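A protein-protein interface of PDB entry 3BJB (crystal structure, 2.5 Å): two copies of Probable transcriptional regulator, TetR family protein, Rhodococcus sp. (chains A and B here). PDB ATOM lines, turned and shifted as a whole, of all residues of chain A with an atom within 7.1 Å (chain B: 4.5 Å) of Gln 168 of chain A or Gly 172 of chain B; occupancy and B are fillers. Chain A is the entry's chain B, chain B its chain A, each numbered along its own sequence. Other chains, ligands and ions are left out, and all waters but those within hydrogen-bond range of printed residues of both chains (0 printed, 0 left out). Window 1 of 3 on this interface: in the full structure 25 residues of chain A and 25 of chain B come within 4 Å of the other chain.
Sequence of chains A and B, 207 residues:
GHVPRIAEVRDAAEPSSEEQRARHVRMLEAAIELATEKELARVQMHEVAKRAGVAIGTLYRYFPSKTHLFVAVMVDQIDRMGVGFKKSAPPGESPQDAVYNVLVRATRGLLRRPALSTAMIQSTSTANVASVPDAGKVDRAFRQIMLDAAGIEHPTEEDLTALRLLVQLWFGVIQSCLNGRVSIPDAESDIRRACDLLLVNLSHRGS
O of Gly 172 of chain B sits close to OE1 of Gln 168 of chain A (3.4 Å).
The side-chain hydroxyl (OG) of Ser 176 of chain B sits at hydrogen-bond distance from the side-chain amide oxygen (OE1) of Gln 168 of chain A.
The side-chain hydroxyl of Ser 176 of chain B sits at hydrogen-bond distance from the backbone carbonyl oxygen of Gly 172 of chain B (3.2 Å).
Leu 165 of chain A touches Leu 169 of chain B (O to CD1, 3.4 Å).
Gln 168 of chain A touches Leu 169 of chain B (CB to CD1, 3.6 Å).
CD1 of Leu 169 of chain A touches CB of Gln 168 of chain B, at 3.8 Å.
Leu 169 of chain B touches Leu 169 of chain A (CD1 to N, 3.7 Å).
O of Gly 172 of chain A touches NE2 of Gln 168 of chain B, at 3.6 Å.
CG2 of Val 173 of chain A touches OE1 of Gln 168 of chain B (3.8 Å).
Gln 175 of chain B touches Gln 175 of chain A (OE1 to OE1, 3.9 Å).
Printed residues of chain B within 4 Å of Leu 165 of chain A: Leu 169 (3.4 Å).
Leu 166 of chain A touches none of the printed residues of chain B.
Gln 168 of chain A touches three residues of chain B.
Trp 170 of chain A touches none of the printed residues of chain B.
Of the printed residues of chain B, Gly 172 of chain A touches Gln 168 (3.6 Å).
Of the printed residues of chain A, Gln 168 of chain B touches Leu 169, Gly 172 and Val 173.
Of the printed residues of chain A, Gly 172 of chain B touches Gln 168 (3.1 Å).
Printed residues of chain A within 4 Å of Ser 176 of chain B: Gln 168.
Printed residues of chain A that touch a printed residue of chain B: Leu 165, Gln 168, Leu 169, Gly 172, Val 173 and Gln 175.
Hydrophobic or aromatic side chains of chain A that line the printed part of chain B: Leu 165, Leu 169 and Val 173.
Of the 9 printed residues of chain B, 5 touch a printed residue of chain A.
Printed residues of chain B that touch a printed residue of chain A: Gln 168, Leu 169, Gly 172, Gln 175 and Ser 176.
Hydrophobic or aromatic side chains of chain B that line the printed part of chain A: Leu 169.
Along chain B the printed residues that touch a printed residue of chain A span positions 168 to 176.
Among the printed residues, 9 pairs touch across the chains.
Among the printed residues, no Asp or Glu carboxylate lies within 4 Å of a Lys or Arg side-chain nitrogen of the other chain.
Gln 168 of chain A touches Leu 169 of chain B, and with the chains exchanged Leu 169 of chain A touches Gln 168 of chain B.
Gln 168 of chain A touches Gly 172 of chain B, and with the chains exchanged Gly 172 of chain A touches Gln 168 of chain B.
Leu 169 of chain A touches its own counterpart, Leu 169 of chain B.
Val 173 of chain A touches Gln 168 of chain B, but with the chains exchanged Gln 168 of chain A does not touch Val 173 of chain B (4.1 Å).
Of the 9 pairs that touch across the chains among the printed residues, 6 have their exchanged pair printed and touching as well.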
ATOM      1  N   THR A 124      -8.129  -8.298  10.843  1.00  0.00           N
ATOM      2  CA  THR A 124      -8.949  -9.136   9.932  1.00  0.00           C
ATOM      3  C   THR A 124      -8.130 -10.111   9.055  1.00  0.00           C
ATOM      4  O   THR A 124      -8.616 -11.162   8.642  1.00  0.00           O
ATOM      5  CB  THR A 124      -9.833  -8.206   9.096  1.00  0.00           C
ATOM      6  OG1 THR A 124     -10.823  -7.647   9.967  1.00  0.00           O
ATOM      7  CG2 THR A 124     -10.496  -8.926   7.923  1.00  0.00           C
ATOM      8  N   ASP A 139     -17.077  -9.828   5.957  1.00  0.00           N
ATOM      9  CA  ASP A 139     -17.285 -10.186   4.560  1.00  0.00           C
ATOM     10  C   ASP A 139     -18.757 -10.009   4.205  1.00  0.00           C
ATOM     11  O   ASP A 139     -19.073  -9.440   3.170  1.00  0.00           O
ATOM     12  CB  ASP A 139     -16.893 -11.640   4.301  1.00  0.00           C
ATOM     13  CG  ASP A 139     -15.636 -12.046   5.038  1.00  0.00           C
ATOM     14  OD1 ASP A 139     -14.758 -11.158   5.293  1.00  0.00           O
ATOM     15  OD2 ASP A 139     -15.551 -13.257   5.384  1.00  0.00           O
ATOM     16  N   PHE A 142     -20.046  -6.388   4.331  1.00  0.00           N
ATOM     17  CA  PHE A 142     -19.486  -5.682   3.215  1.00  0.00           C
ATOM     18  C   PHE A 142     -20.237  -6.023   1.957  1.00  0.00           C
ATOM     19  O   PHE A 142     -20.950  -5.196   1.394  1.00  0.00           O
ATOM     20  CB  PHE A 142     -18.009  -6.006   3.083  1.00  0.00           C
ATOM     21  CG  PHE A 142     -17.220  -4.857   2.626  1.00  0.00           C
ATOM     22  CD1 PHE A 142     -16.135  -5.031   1.788  1.00  0.00           C
ATOM     23  CD2 PHE A 142     -17.602  -3.570   2.988  1.00  0.00           C
ATOM     24  CE1 PHE A 142     -15.401  -3.916   1.316  1.00  0.00           C
ATOM     25  CE2 PHE A 142     -16.896  -2.427   2.529  1.00  0.00           C
ATOM     26  CZ  PHE A 142     -15.781  -2.595   1.697  1.00  0.00           C
ATOM     27  N   ALA A 162     -17.665 -13.166  -7.707  1.00  0.00           N
ATOM     28  CA  ALA A 162     -17.052 -11.910  -8.208  1.00  0.00           C
ATOM     29  C   ALA A 162     -16.793 -10.897  -7.102  1.00  0.00           C
ATOM     30  O   ALA A 162     -15.697 -10.359  -6.978  1.00  0.00           O
ATOM     31  CB  ALA A 162     -17.890 -11.296  -9.323  1.00  0.00           C
ATOM     32  N   LEU A 163     -17.797 -10.673  -6.265  1.00  0.00           N
ATOM     33  CA  LEU A 163     -17.665  -9.741  -5.152  1.00  0.00           C
ATOM     34  C   LEU A 163     -16.767 -10.245  -4.033  1.00  0.00           C
ATOM     35  O   LEU A 163     -16.313  -9.465  -3.226  1.00  0.00           O
ATOM     36  CB  LEU A 163     -19.038  -9.389  -4.595  1.00  0.00           C
ATOM     37  CG  LEU A 163     -19.919  -8.618  -5.576  1.00  0.00           C
ATOM     38  CD1 LEU A 163     -21.373  -8.697  -5.133  1.00  0.00           C
ATOM     39  CD2 LEU A 163     -19.455  -7.166  -5.726  1.00  0.00           C
ATOM     40  N   ARG A 164     -16.535 -11.547  -3.952  1.00  0.00           N
ATOM     41  CA  ARG A 164     -15.657 -12.059  -2.906  1.00  0.00           C
ATOM     42  C   ARG A 164     -14.241 -11.813  -3.405  1.00  0.00           C
ATOM     43  O   ARG A 164     -13.400 -11.324  -2.664  1.00  0.00           O
ATOM     44  CB  ARG A 164     -15.930 -13.547  -2.624  1.00  0.00           C
ATOM     45  CG  ARG A 164     -15.565 -13.991  -1.175  1.00  0.00           C
ATOM     46  CD  ARG A 164     -15.369 -15.523  -1.001  1.00  0.00           C
ATOM     47  NE  ARG A 164     -16.146 -16.233  -2.006  1.00  0.00           N
ATOM     48  CZ  ARG A 164     -15.606 -16.920  -3.002  1.00  0.00           C
ATOM     49  NH1 ARG A 164     -14.289 -17.014  -3.078  1.00  0.00           N
ATOM     50  NH2 ARG A 164     -16.376 -17.505  -3.907  1.00  0.00           N
ATOM     51  N   LEU A 165     -14.007 -12.104  -4.687  1.00  0.00           N
ATOM     52  CA  LEU A 165     -12.761 -11.706  -5.356  1.00  0.00           C
ATOM     53  C   LEU A 165     -12.445 -10.183  -5.271  1.00  0.00           C
ATOM     54  O   LEU A 165     -11.292  -9.794  -5.085  1.00  0.00           O
ATOM     55  CB  LEU A 165     -12.770 -12.176  -6.810  1.00  0.00           C
ATOM     56  CG  LEU A 165     -12.812 -13.696  -7.068  1.00  0.00           C
ATOM     57  CD1 LEU A 165     -12.871 -13.989  -8.575  1.00  0.00           C
ATOM     58  CD2 LEU A 165     -11.638 -14.410  -6.479  1.00  0.00           C
ATOM     59  N   LEU A 166     -13.460  -9.329  -5.419  1.00  0.00           N
ATOM     60  CA  LEU A 166     -13.239  -7.891  -5.313  1.00  0.00           C
ATOM     61  C   LEU A 166     -12.787  -7.485  -3.903  1.00  0.00           C
ATOM     62  O   LEU A 166     -11.678  -6.972  -3.764  1.00  0.00           O
ATOM     63  CB  LEU A 166     -14.456  -7.091  -5.773  1.00  0.00           C
ATOM     64  CG  LEU A 166     -14.361  -5.569  -5.965  1.00  0.00           C
ATOM     65  CD1 LEU A 166     -13.251  -5.139  -6.923  1.00  0.00           C
ATOM     66  CD2 LEU A 166     -15.708  -4.981  -6.410  1.00  0.00           C
ATOM     67  N   VAL A 167     -13.587  -7.743  -2.856  1.00  0.00           N
ATOM     68  CA  VAL A 167     -13.171  -7.259  -1.514  1.00  0.00           C
ATOM     69  C   VAL A 167     -11.825  -7.843  -1.122  1.00  0.00           C
ATOM     70  O   VAL A 167     -11.097  -7.259  -0.322  1.00  0.00           O
ATOM     71  CB  VAL A 167     -14.222  -7.408  -0.351  1.00  0.00           C
ATOM     72  CG1 VAL A 167     -15.647  -7.433  -0.861  1.00  0.00           C
ATOM     73  CG2 VAL A 167     -13.938  -8.605   0.536  1.00  0.00           C
ATOM     74  N   GLN A 168     -11.493  -8.984  -1.719  1.00  0.00           N
ATOM     75  CA  GLN A 168     -10.202  -9.638  -1.469  1.00  0.00           C
ATOM     76  C   GLN A 168      -9.084  -8.813  -2.069  1.00  0.00           C
ATOM     77  O   GLN A 168      -8.283  -8.240  -1.334  1.00  0.00           O
ATOM     78  CB  GLN A 168     -10.180 -11.117  -1.930  1.00  0.00           C
ATOM     79  CG  GLN A 168     -10.202 -12.154  -0.743  1.00  0.00           C
ATOM     80  CD  GLN A 168      -9.555 -11.613   0.589  1.00  0.00           C
ATOM     81  OE1 GLN A 168      -8.364 -11.849   0.870  1.00  0.00           O
ATOM     82  NE2 GLN A 168     -10.354 -10.878   1.392  1.00  0.00           N
ATOM     83  N   LEU A 169      -9.078  -8.713  -3.394  1.00  0.00           N
ATOM     84  CA  LEU A 169      -8.259  -7.741  -4.111  1.00  0.00           C
ATOM     85  C   LEU A 169      -8.256  -6.339  -3.466  1.00  0.00           C
ATOM     86  O   LEU A 169      -7.245  -5.648  -3.477  1.00  0.00           O
ATOM     87  CB  LEU A 169      -8.709  -7.656  -5.558  1.00  0.00           C
ATOM     88  CG  LEU A 169      -8.080  -6.618  -6.481  1.00  0.00           C
ATOM     89  CD1 LEU A 169      -6.593  -6.533  -6.324  1.00  0.00           C
ATOM     90  CD2 LEU A 169      -8.387  -7.029  -7.894  1.00  0.00           C
ATOM     91  N   TRP A 170      -9.371  -5.930  -2.884  1.00  0.00           N
ATOM     92  CA  TRP A 170      -9.486  -4.585  -2.378  1.00  0.00           C
ATOM     93  C   TRP A 170      -8.669  -4.438  -1.113  1.00  0.00           C
ATOM     94  O   TRP A 170      -7.838  -3.534  -1.018  1.00  0.00           O
ATOM     95  CB  TRP A 170     -10.938  -4.224  -2.128  1.00  0.00           C
ATOM     96  CG  TRP A 170     -11.081  -2.888  -1.522  1.00  0.00           C
ATOM     97  CD1 TRP A 170     -10.851  -1.694  -2.124  1.00  0.00           C
ATOM     98  CD2 TRP A 170     -11.479  -2.601  -0.190  1.00  0.00           C
ATOM     99  NE1 TRP A 170     -11.075  -0.682  -1.258  1.00  0.00           N
ATOM    100  CE2 TRP A 170     -11.477  -1.200  -0.058  1.00  0.00           C
ATOM    101  CE3 TRP A 170     -11.848  -3.395   0.908  1.00  0.00           C
ATOM    102  CZ2 TRP A 170     -11.818  -0.554   1.127  1.00  0.00           C
ATOM    103  CZ3 TRP A 170     -12.193  -2.763   2.101  1.00  0.00           C
ATOM    104  CH2 TRP A 170     -12.172  -1.342   2.198  1.00  0.00           C
ATOM    105  N   PHE A 171      -8.911  -5.342  -0.155  1.00  0.00           N
ATOM    106  CA  PHE A 171      -8.118  -5.416   1.075  1.00  0.00           C
ATOM    107  C   PHE A 171      -6.634  -5.354   0.784  1.00  0.00           C
ATOM    108  O   PHE A 171      -5.902  -4.719   1.517  1.00  0.00           O
ATOM    109  CB  PHE A 171      -8.412  -6.694   1.871  1.00  0.00           C
ATOM    110  CG  PHE A 171      -9.379  -6.490   2.981  1.00  0.00           C
ATOM    111  CD1 PHE A 171      -8.964  -6.572   4.302  1.00  0.00           C
ATOM    112  CD2 PHE A 171     -10.730  -6.195   2.710  1.00  0.00           C
ATOM    113  CE1 PHE A 171      -9.884  -6.362   5.347  1.00  0.00           C
ATOM    114  CE2 PHE A 171     -11.675  -5.992   3.753  1.00  0.00           C
ATOM    115  CZ  PHE A 171     -11.248  -6.075   5.067  1.00  0.00           C
ATOM    116  N   GLY A 172      -6.203  -6.022  -0.275  1.00  0.00           N
ATOM    117  CA  GLY A 172      -4.793  -6.004  -0.640  1.00  0.00           C
ATOM    118  C   GLY A 172      -4.326  -4.607  -1.015  1.00  0.00           C
ATOM    119  O   GLY A 172      -3.270  -4.163  -0.564  1.00  0.00           O
ATOM    120  N   VAL A 173      -5.144  -3.906  -1.811  1.00  0.00           N
ATOM    121  CA  VAL A 173      -4.780  -2.601  -2.312  1.00  0.00           C
ATOM    122  C   VAL A 173      -4.639  -1.623  -1.158  1.00  0.00           C
ATOM    123  O   VAL A 173      -3.680  -0.803  -1.138  1.00  0.00           O
ATOM    124  CB  VAL A 173      -5.819  -2.074  -3.316  1.00  0.00           C
ATOM    125  CG1 VAL A 173      -5.393  -0.730  -3.848  1.00  0.00           C
ATOM    126  CG2 VAL A 173      -6.071  -3.125  -4.468  1.00  0.00           C
ATOM    127  N   GLN A 175      -4.027  -2.346   2.076  1.00  0.00           N
ATOM    128  CA  GLN A 175      -2.928  -2.755   2.909  1.00  0.00           C
ATOM    129  C   GLN A 175      -1.666  -2.163   2.288  1.00  0.00           C
ATOM    130  O   GLN A 175      -0.821  -1.552   2.958  1.00  0.00           O
ATOM    131  CB  GLN A 175      -2.855  -4.286   2.900  1.00  0.00           C
ATOM    132  CG  GLN A 175      -2.562  -4.963   4.254  1.00  0.00           C
ATOM    133  CD  GLN A 175      -2.994  -6.467   4.271  1.00  0.00           C
ATOM    134  OE1 GLN A 175      -3.456  -6.998   3.261  1.00  0.00           O
ATOM    135  NE2 GLN A 175      -2.825  -7.138   5.432  1.00  0.00           N
ATOM    136  N   GLN B 168      -1.895  -9.218  -6.291  1.00  0.00           N
ATOM    137  CA  GLN B 168      -2.548  -8.664  -5.121  1.00  0.00           C
ATOM    138  C   GLN B 168      -3.746  -9.491  -4.685  1.00  0.00           C
ATOM    139  O   GLN B 168      -3.879  -9.791  -3.508  1.00  0.00           O
ATOM    140  CB  GLN B 168      -2.959  -7.227  -5.377  1.00  0.00           C
ATOM    141  CG  GLN B 168      -1.784  -6.303  -5.437  1.00  0.00           C
ATOM    142  CD  GLN B 168      -2.166  -4.898  -5.111  1.00  0.00           C
ATOM    143  OE1 GLN B 168      -2.768  -4.198  -5.935  1.00  0.00           O
ATOM    144  NE2 GLN B 168      -1.825  -4.459  -3.900  1.00  0.00           N
ATOM    145  N   LEU B 169      -4.591  -9.897  -5.626  1.00  0.00           N
ATOM    146  CA  LEU B 169      -5.693 -10.800  -5.293  1.00  0.00           C
ATOM    147  C   LEU B 169      -5.140 -12.116  -4.749  1.00  0.00           C
ATOM    148  O   LEU B 169      -5.589 -12.598  -3.719  1.00  0.00           O
ATOM    149  CB  LEU B 169      -6.614 -11.045  -6.505  1.00  0.00           C
ATOM    150  CG  LEU B 169      -7.728 -12.101  -6.369  1.00  0.00           C
ATOM    151  CD1 LEU B 169      -8.579 -11.915  -5.096  1.00  0.00           C
ATOM    152  CD2 LEU B 169      -8.633 -12.092  -7.559  1.00  0.00           C
ATOM    153  N   TRP B 170      -4.156 -12.681  -5.444  1.00  0.00           N
ATOM    154  CA  TRP B 170      -3.550 -13.957  -5.068  1.00  0.00           C
ATOM    155  C   TRP B 170      -2.988 -13.955  -3.650  1.00  0.00           C
ATOM    156  O   TRP B 170      -3.113 -14.937  -2.940  1.00  0.00           O
ATOM    157  CB  TRP B 170      -2.476 -14.337  -6.088  1.00  0.00           C
ATOM    158  CG  TRP B 170      -1.689 -15.545  -5.729  1.00  0.00           C
ATOM    159  CD1 TRP B 170      -1.955 -16.818  -6.083  1.00  0.00           C
ATOM    160  CD2 TRP B 170      -0.489 -15.578  -4.953  1.00  0.00           C
ATOM    161  NE1 TRP B 170      -1.006 -17.653  -5.563  1.00  0.00           N
ATOM    162  CE2 TRP B 170      -0.094 -16.905  -4.861  1.00  0.00           C
ATOM    163  CE3 TRP B 170       0.287 -14.598  -4.311  1.00  0.00           C
ATOM    164  CZ2 TRP B 170       1.049 -17.298  -4.159  1.00  0.00           C
ATOM    165  CZ3 TRP B 170       1.426 -14.999  -3.591  1.00  0.00           C
ATOM    166  CH2 TRP B 170       1.787 -16.332  -3.537  1.00  0.00           C
ATOM    167  N   PHE B 171      -2.378 -12.848  -3.237  1.00  0.00           N
ATOM    168  CA  PHE B 171      -2.060 -12.623  -1.826  1.00  0.00           C
ATOM    169  C   PHE B 171      -3.275 -12.764  -0.937  1.00  0.00           C
ATOM    170  O   PHE B 171      -3.258 -13.550   0.013  1.00  0.00           O
ATOM    171  CB  PHE B 171      -1.478 -11.231  -1.590  1.00  0.00           C
ATOM    172  CG  PHE B 171      -0.022 -11.170  -1.801  1.00  0.00           C
ATOM    173  CD1 PHE B 171       0.802 -12.080  -1.177  1.00  0.00           C
ATOM    174  CD2 PHE B 171       0.526 -10.226  -2.658  1.00  0.00           C
ATOM    175  CE1 PHE B 171       2.156 -12.049  -1.380  1.00  0.00           C
ATOM    176  CE2 PHE B 171       1.895 -10.183  -2.888  1.00  0.00           C
ATOM    177  CZ  PHE B 171       2.718 -11.092  -2.241  1.00  0.00           C
ATOM    178  N   GLY B 172      -4.313 -11.984  -1.234  1.00  0.00           N
ATOM    179  CA  GLY B 172      -5.578 -12.112  -0.533  1.00  0.00           C
ATOM    180  C   GLY B 172      -5.905 -13.589  -0.425  1.00  0.00           C
ATOM    181  O   GLY B 172      -5.942 -14.163   0.676  1.00  0.00           O
ATOM    182  N   VAL B 173      -6.079 -14.229  -1.567  1.00  0.00           N
ATOM    183  CA  VAL B 173      -6.407 -15.615  -1.533  1.00  0.00           C
ATOM    184  C   VAL B 173      -5.459 -16.412  -0.626  1.00  0.00           C
ATOM    185  O   VAL B 173      -5.908 -17.230   0.175  1.00  0.00           O
ATOM    186  CB  VAL B 173      -6.508 -16.239  -2.982  1.00  0.00           C
ATOM    187  CG1 VAL B 173      -6.622 -17.734  -2.901  1.00  0.00           C
ATOM    188  CG2 VAL B 173      -7.687 -15.616  -3.757  1.00  0.00           C
ATOM    189  N   ILE B 174      -4.159 -16.219  -0.757  1.00  0.00           N
ATOM    190  CA  ILE B 174      -3.248 -17.040   0.028  1.00  0.00           C
ATOM    191  C   ILE B 174      -3.507 -16.824   1.529  1.00  0.00           C
ATOM    192  O   ILE B 174      -3.682 -17.799   2.263  1.00  0.00           O
ATOM    193  CB  ILE B 174      -1.786 -16.873  -0.435  1.00  0.00           C
ATOM    194  CG1 ILE B 174      -1.351 -18.128  -1.149  1.00  0.00           C
ATOM    195  CG2 ILE B 174      -0.837 -16.727   0.694  1.00  0.00           C
ATOM    196  CD1 ILE B 174      -2.044 -18.350  -2.445  1.00  0.00           C
ATOM    197  N   GLN B 175      -3.587 -15.559   1.953  1.00  0.00           N
ATOM    198  CA  GLN B 175      -3.926 -15.173   3.344  1.00  0.00           C
ATOM    199  C   GLN B 175      -5.286 -15.803   3.780  1.00  0.00           C
ATOM    200  O   GLN B 175      -5.351 -16.533   4.759  1.00  0.00           O
ATOM    201  CB  GLN B 175      -3.899 -13.621   3.491  1.00  0.00           C
ATOM    202  CG  GLN B 175      -3.409 -13.083   4.845  1.00  0.00           C
ATOM    203  CD  GLN B 175      -2.712 -11.664   4.803  1.00  0.00           C
ATOM    204  OE1 GLN B 175      -3.053 -10.766   4.003  1.00  0.00           O
ATOM    205  NE2 GLN B 175      -1.734 -11.481   5.702  1.00  0.00           N
ATOM    206  N   SER B 176      -6.343 -15.546   3.011  1.00  0.00           N
ATOM    207  CA  SER B 176      -7.647 -16.174   3.197  1.00  0.00           C
ATOM    208  C   SER B 176      -7.542 -17.679   3.308  1.00  0.00           C
ATOM    209  O   SER B 176      -8.397 -18.317   3.931  1.00  0.00           O
ATOM    210  CB  SER B 176      -8.579 -15.871   2.013  1.00  0.00           C
ATOM    211  OG  SER B 176      -8.867 -14.488   1.905  1.00  0.00           O
